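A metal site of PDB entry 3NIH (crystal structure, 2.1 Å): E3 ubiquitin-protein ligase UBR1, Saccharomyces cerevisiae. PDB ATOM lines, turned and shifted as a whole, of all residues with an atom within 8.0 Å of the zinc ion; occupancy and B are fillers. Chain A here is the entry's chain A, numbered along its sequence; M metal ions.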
ATOM      1  N   ARG A  23      23.572 -21.818  24.533  1.00  0.00           N
ATOM      2  CA  ARG A  23      24.750 -21.949  25.386  1.00  0.00           C
ATOM      3  C   ARG A  23      25.079 -23.418  25.601  1.00  0.00           C
ATOM      4  O   ARG A  23      24.205 -24.290  25.489  1.00  0.00           O
ATOM      5  CB  ARG A  23      24.504 -21.282  26.742  1.00  0.00           C
ATOM      6  CG  ARG A  23      24.445 -19.780  26.699  1.00  0.00           C
ATOM      7  CD  ARG A  23      24.146 -19.196  28.070  1.00  0.00           C
ATOM      8  NE  ARG A  23      22.843 -19.635  28.572  1.00  0.00           N
ATOM      9  CZ  ARG A  23      22.063 -18.923  29.386  1.00  0.00           C
ATOM     10  NH1 ARG A  23      22.448 -17.717  29.816  1.00  0.00           N
ATOM     11  NH2 ARG A  23      20.899 -19.418  29.784  1.00  0.00           N
ATOM     12  N   CYS A  24      26.327 -23.691  25.926  1.00  0.00           N
ATOM     13  CA  CYS A  24      26.750 -25.058  26.176  1.00  0.00           C
ATOM     14  C   CYS A  24      27.598 -25.101  27.435  1.00  0.00           C
ATOM     15  O   CYS A  24      28.615 -24.426  27.515  1.00  0.00           O
ATOM     16  CB  CYS A  24      27.519 -25.609  24.985  1.00  0.00           C
ATOM     17  SG  CYS A  24      28.009 -27.326  25.176  1.00  0.00           S
ATOM     18  N   HIS A  25      27.148 -25.881  28.415  1.00  0.00           N
ATOM     19  CA  HIS A  25      27.853 -25.989  29.687  1.00  0.00           C
ATOM     20  C   HIS A  25      29.330 -26.376  29.506  1.00  0.00           C
ATOM     21  O   HIS A  25      30.200 -25.761  30.122  1.00  0.00           O
ATOM     22  CB  HIS A  25      27.164 -27.000  30.611  1.00  0.00           C
ATOM     23  CG  HIS A  25      27.856 -27.171  31.934  1.00  0.00           C
ATOM     24  ND1 HIS A  25      27.733 -26.258  32.963  1.00  0.00           N
ATOM     25  CD2 HIS A  25      28.704 -28.128  32.381  1.00  0.00           C
ATOM     26  CE1 HIS A  25      28.469 -26.653  33.984  1.00  0.00           C
ATOM     27  NE2 HIS A  25      29.067 -27.784  33.661  1.00  0.00           N
ATOM     28  N   GLU A  26      29.579 -27.363  28.662  1.00  0.00           N
ATOM     29  CA  GLU A  26      30.943 -27.845  28.381  1.00  0.00           C
ATOM     30  C   GLU A  26      31.770 -26.860  27.551  1.00  0.00           C
ATOM     31  O   GLU A  26      32.891 -26.519  27.939  1.00  0.00           O
ATOM     32  CB  GLU A  26      30.914 -29.216  27.694  1.00  0.00           C
ATOM     33  CG  GLU A  26      30.400 -30.369  28.556  1.00  0.00           C
ATOM     34  CD  GLU A  26      28.908 -30.307  28.868  1.00  0.00           C
ATOM     35  OE1 GLU A  26      28.133 -29.873  27.995  1.00  0.00           O
ATOM     36  OE2 GLU A  26      28.512 -30.705  29.986  1.00  0.00           O
ATOM     37  N   CYS A  27      31.218 -26.402  26.431  1.00  0.00           N
ATOM     38  CA  CYS A  27      31.959 -25.599  25.461  1.00  0.00           C
ATOM     39  C   CYS A  27      32.154 -24.131  25.873  1.00  0.00           C
ATOM     40  O   CYS A  27      33.182 -23.545  25.558  1.00  0.00           O
ATOM     41  CB  CYS A  27      31.308 -25.671  24.070  1.00  0.00           C
ATOM     42  SG  CYS A  27      30.984 -27.383  23.511  1.00  0.00           S
ATOM     43  N   GLY A  28      31.171 -23.554  26.559  1.00  0.00           N
ATOM     44  CA  GLY A  28      31.242 -22.166  26.999  1.00  0.00           C
ATOM     45  C   GLY A  28      32.181 -21.966  28.179  1.00  0.00           C
ATOM     46  O   GLY A  28      32.181 -22.764  29.120  1.00  0.00           O
ATOM     47  N   LEU A  35      25.690 -18.599  21.345  1.00  0.00           N
ATOM     48  CA  LEU A  35      25.687 -18.754  19.890  1.00  0.00           C
ATOM     49  C   LEU A  35      24.303 -18.442  19.359  1.00  0.00           C
ATOM     50  O   LEU A  35      23.303 -18.778  19.990  1.00  0.00           O
ATOM     51  CB  LEU A  35      26.023 -20.194  19.517  1.00  0.00           C
ATOM     52  CG  LEU A  35      27.453 -20.651  19.866  1.00  0.00           C
ATOM     53  CD1 LEU A  35      27.552 -22.163  19.832  1.00  0.00           C
ATOM     54  CD2 LEU A  35      28.417 -20.020  18.878  1.00  0.00           C
ATOM     55  N   PHE A  40      25.147 -21.907  15.708  1.00  0.00           N
ATOM     56  CA  PHE A  40      25.090 -23.150  16.476  1.00  0.00           C
ATOM     57  C   PHE A  40      24.999 -24.386  15.582  1.00  0.00           C
ATOM     58  O   PHE A  40      24.080 -24.527  14.756  1.00  0.00           O
ATOM     59  CB  PHE A  40      23.932 -23.122  17.485  1.00  0.00           C
ATOM     60  CG  PHE A  40      23.783 -24.411  18.288  1.00  0.00           C
ATOM     61  CD1 PHE A  40      24.505 -24.606  19.463  1.00  0.00           C
ATOM     62  CD2 PHE A  40      22.906 -25.399  17.866  1.00  0.00           C
ATOM     63  CE1 PHE A  40      24.352 -25.789  20.201  1.00  0.00           C
ATOM     64  CE2 PHE A  40      22.752 -26.596  18.590  1.00  0.00           C
ATOM     65  CZ  PHE A  40      23.485 -26.784  19.758  1.00  0.00           C
ATOM     66  N   ASN A  41      25.973 -25.273  15.769  1.00  0.00           N
ATOM     67  CA  ASN A  41      26.039 -26.521  15.025  1.00  0.00           C
ATOM     68  C   ASN A  41      25.834 -27.693  15.982  1.00  0.00           C
ATOM     69  O   ASN A  41      26.659 -27.894  16.875  1.00  0.00           O
ATOM     70  CB  ASN A  41      27.403 -26.625  14.316  1.00  0.00           C
ATOM     71  CG  ASN A  41      27.421 -27.669  13.209  1.00  0.00           C
ATOM     72  OD1 ASN A  41      26.680 -28.658  13.241  1.00  0.00           O
ATOM     73  ND2 ASN A  41      28.269 -27.450  12.217  1.00  0.00           N
ATOM     74  N   PRO A  42      24.724 -28.449  15.817  1.00  0.00           N
ATOM     75  CA  PRO A  42      24.461 -29.584  16.696  1.00  0.00           C
ATOM     76  C   PRO A  42      25.612 -30.578  16.715  1.00  0.00           C
ATOM     77  O   PRO A  42      25.836 -31.257  17.728  1.00  0.00           O
ATOM     78  CB  PRO A  42      23.219 -30.234  16.070  1.00  0.00           C
ATOM     79  CG  PRO A  42      22.559 -29.139  15.304  1.00  0.00           C
ATOM     80  CD  PRO A  42      23.669 -28.268  14.810  1.00  0.00           C
ATOM     81  N   LYS A  43      26.349 -30.661  15.605  1.00  0.00           N
ATOM     82  CA  LYS A  43      27.485 -31.564  15.447  1.00  0.00           C
ATOM     83  C   LYS A  43      28.628 -31.297  16.422  1.00  0.00           C
ATOM     84  O   LYS A  43      29.410 -32.188  16.735  1.00  0.00           O
ATOM     85  CB  LYS A  43      27.990 -31.527  14.008  1.00  0.00           C
ATOM     86  CG  LYS A  43      27.145 -32.345  13.026  1.00  0.00           C
ATOM     87  CD  LYS A  43      27.258 -31.825  11.593  1.00  0.00           C
ATOM     88  CE  LYS A  43      28.657 -32.014  11.013  1.00  0.00           C
ATOM     89  NZ  LYS A  43      28.785 -31.366   9.692  1.00  0.00           N
ATOM     90  N   ASP A  44      28.724 -30.050  16.892  1.00  0.00           N
ATOM     91  CA  ASP A  44      29.722 -29.657  17.873  1.00  0.00           C
ATOM     92  C   ASP A  44      29.351 -30.103  19.281  1.00  0.00           C
ATOM     93  O   ASP A  44      30.222 -30.158  20.166  1.00  0.00           O
ATOM     94  CB  ASP A  44      29.913 -28.129  17.866  1.00  0.00           C
ATOM     95  CG  ASP A  44      30.605 -27.630  16.609  1.00  0.00           C
ATOM     96  OD1 ASP A  44      31.462 -28.349  16.057  1.00  0.00           O
ATOM     97  OD2 ASP A  44      30.284 -26.489  16.185  1.00  0.00           O
ATOM     98  N   HIS A  45      28.076 -30.410  19.507  1.00  0.00           N
ATOM     99  CA  HIS A  45      27.538 -30.553  20.854  1.00  0.00           C
ATOM    100  C   HIS A  45      26.714 -31.820  21.114  1.00  0.00           C
ATOM    101  O   HIS A  45      25.718 -31.787  21.855  1.00  0.00           O
ATOM    102  CB  HIS A  45      26.724 -29.307  21.224  1.00  0.00           C
ATOM    103  CG  HIS A  45      27.389 -28.014  20.857  1.00  0.00           C
ATOM    104  ND1 HIS A  45      28.415 -27.474  21.602  1.00  0.00           N
ATOM    105  CD2 HIS A  45      27.192 -27.173  19.821  1.00  0.00           C
ATOM    106  CE1 HIS A  45      28.816 -26.335  21.043  1.00  0.00           C
ATOM    107  NE2 HIS A  45      28.093 -26.139  19.953  1.00  0.00           N
ATOM    108  N   VAL A  46      27.135 -32.939  20.527  1.00  0.00           N
ATOM    109  CA  VAL A  46      26.451 -34.226  20.746  1.00  0.00           C
ATOM    110  C   VAL A  46      26.561 -34.656  22.208  1.00  0.00           C
ATOM    111  O   VAL A  46      27.664 -34.744  22.763  1.00  0.00           O
ATOM    112  CB  VAL A  46      26.956 -35.331  19.785  1.00  0.00           C
ATOM    113  CG1 VAL A  46      26.191 -36.643  20.004  1.00  0.00           C
ATOM    114  CG2 VAL A  46      26.817 -34.872  18.337  1.00  0.00           C
ATOM    115  N   ASN A  47      25.395 -34.893  22.830  1.00  0.00           N
ATOM    116  CA  ASN A  47      25.268 -35.257  24.247  1.00  0.00           C
ATOM    117  C   ASN A  47      25.920 -34.269  25.219  1.00  0.00           C
ATOM    118  O   ASN A  47      26.147 -34.586  26.390  1.00  0.00           O
ATOM    119  CB  ASN A  47      25.749 -36.696  24.498  1.00  0.00           C
ATOM    120  CG  ASN A  47      24.751 -37.744  23.941  1.00  0.00           C
ATOM    121  OD1 ASN A  47      25.153 -38.820  23.396  1.00  0.00           O
ATOM    122  ND2 ASN A  47      23.451 -37.429  24.076  1.00  0.00           N
ATOM    123  N   HIS A  48      26.232 -33.076  24.708  1.00  0.00           N
ATOM    124  CA  HIS A  48      26.611 -31.930  25.527  1.00  0.00           C
ATOM    125  C   HIS A  48      25.376 -31.386  26.226  1.00  0.00           C
ATOM    126  O   HIS A  48      24.233 -31.753  25.894  1.00  0.00           O
ATOM    127  CB  HIS A  48      27.283 -30.847  24.659  1.00  0.00           C
ATOM    128  CG  HIS A  48      28.704 -31.169  24.314  1.00  0.00           C
ATOM    129  ND1 HIS A  48      29.577 -30.232  23.789  1.00  0.00           N
ATOM    130  CD2 HIS A  48      29.428 -32.301  24.458  1.00  0.00           C
ATOM    131  CE1 HIS A  48      30.757 -30.784  23.599  1.00  0.00           C
ATOM    132  NE2 HIS A  48      30.693 -32.044  24.000  1.00  0.00           N
ATOM    133  N   HIS A  49      25.581 -30.535  27.223  1.00  0.00           N
ATOM    134  CA  HIS A  49      24.455 -29.995  27.951  1.00  0.00           C
ATOM    135  C   HIS A  49      24.115 -28.613  27.426  1.00  0.00           C
ATOM    136  O   HIS A  49      24.581 -27.601  27.936  1.00  0.00           O
ATOM    137  CB  HIS A  49      24.711 -30.027  29.460  1.00  0.00           C
ATOM    138  CG  HIS A  49      24.760 -31.418  30.018  1.00  0.00           C
ATOM    139  ND1 HIS A  49      25.880 -32.206  29.943  1.00  0.00           N
ATOM    140  CD2 HIS A  49      23.804 -32.181  30.597  1.00  0.00           C
ATOM    141  CE1 HIS A  49      25.628 -33.387  30.483  1.00  0.00           C
ATOM    142  NE2 HIS A  49      24.373 -33.397  30.890  1.00  0.00           N
ATOM    143  N   VAL A  50      23.293 -28.619  26.372  1.00  0.00           N
ATOM    144  CA  VAL A  50      22.948 -27.416  25.629  1.00  0.00           C
ATOM    145  C   VAL A  50      21.687 -26.772  26.199  1.00  0.00           C
ATOM    146  O   VAL A  50      20.659 -27.416  26.388  1.00  0.00           O
ATOM    147  CB  VAL A  50      22.790 -27.692  24.117  1.00  0.00           C
ATOM    148  CG1 VAL A  50      22.428 -26.397  23.338  1.00  0.00           C
ATOM    149  CG2 VAL A  50      24.082 -28.287  23.568  1.00  0.00           C
ATOM    150  N   TRP A  71      35.184 -19.816  24.251  1.00  0.00           N
ATOM    151  CA  TRP A  71      34.958 -21.245  24.072  1.00  0.00           C
ATOM    152  C   TRP A  71      36.131 -22.109  24.515  1.00  0.00           C
ATOM    153  O   TRP A  71      37.289 -21.704  24.407  1.00  0.00           O
ATOM    154  CB  TRP A  71      34.548 -21.554  22.615  1.00  0.00           C
ATOM    155  CG  TRP A  71      33.416 -20.670  22.180  1.00  0.00           C
ATOM    156  CD1 TRP A  71      33.497 -19.577  21.364  1.00  0.00           C
ATOM    157  CD2 TRP A  71      32.038 -20.753  22.593  1.00  0.00           C
ATOM    158  NE1 TRP A  71      32.261 -18.991  21.220  1.00  0.00           N
ATOM    159  CE2 TRP A  71      31.345 -19.698  21.969  1.00  0.00           C
ATOM    160  CE3 TRP A  71      31.335 -21.637  23.430  1.00  0.00           C
ATOM    161  CZ2 TRP A  71      29.971 -19.485  22.153  1.00  0.00           C
ATOM    162  CZ3 TRP A  71      29.970 -21.439  23.615  1.00  0.00           C
ATOM    163  CH2 TRP A  71      29.298 -20.370  22.977  1.00  0.00           C
ATOM    164  N   SER A  73      36.340 -25.391  23.353  1.00  0.00           N
ATOM    165  CA  SER A  73      36.596 -26.254  22.197  1.00  0.00           C
ATOM    166  C   SER A  73      36.519 -25.442  20.901  1.00  0.00           C
ATOM    167  O   SER A  73      35.850 -24.411  20.872  1.00  0.00           O
ATOM    168  CB  SER A  73      35.599 -27.418  22.172  1.00  0.00           C
ATOM    169  OG  SER A  73      35.775 -28.249  23.298  1.00  0.00           O
ATOM    170  N   LEU A  75      34.905 -24.495  17.619  1.00  0.00           N
ATOM    171  CA  LEU A  75      33.572 -24.659  17.057  1.00  0.00           C
ATOM    172  C   LEU A  75      33.636 -24.648  15.530  1.00  0.00           C
ATOM    173  O   LEU A  75      34.647 -24.276  14.948  1.00  0.00           O
ATOM    174  CB  LEU A  75      32.611 -23.562  17.569  1.00  0.00           C
ATOM    175  CG  LEU A  75      32.257 -23.555  19.072  1.00  0.00           C
ATOM    176  CD1 LEU A  75      31.340 -22.397  19.393  1.00  0.00           C
ATOM    177  CD2 LEU A  75      31.640 -24.870  19.532  1.00  0.00           C
HETATM  178 ZN    ZN M   1      29.045 -28.077  23.452  1.00  0.00          ZN
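The nearest printed residue that does not touch the zinc ion is Asp 44 (4.1 Å).
The zinc ion is bound by ND1 of His 45 (2.0 Å), SG of Cys 27 (2.1 Å), SG of Cys 24 (2.1 Å) and ND1 of His 48 (2.2 Å).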
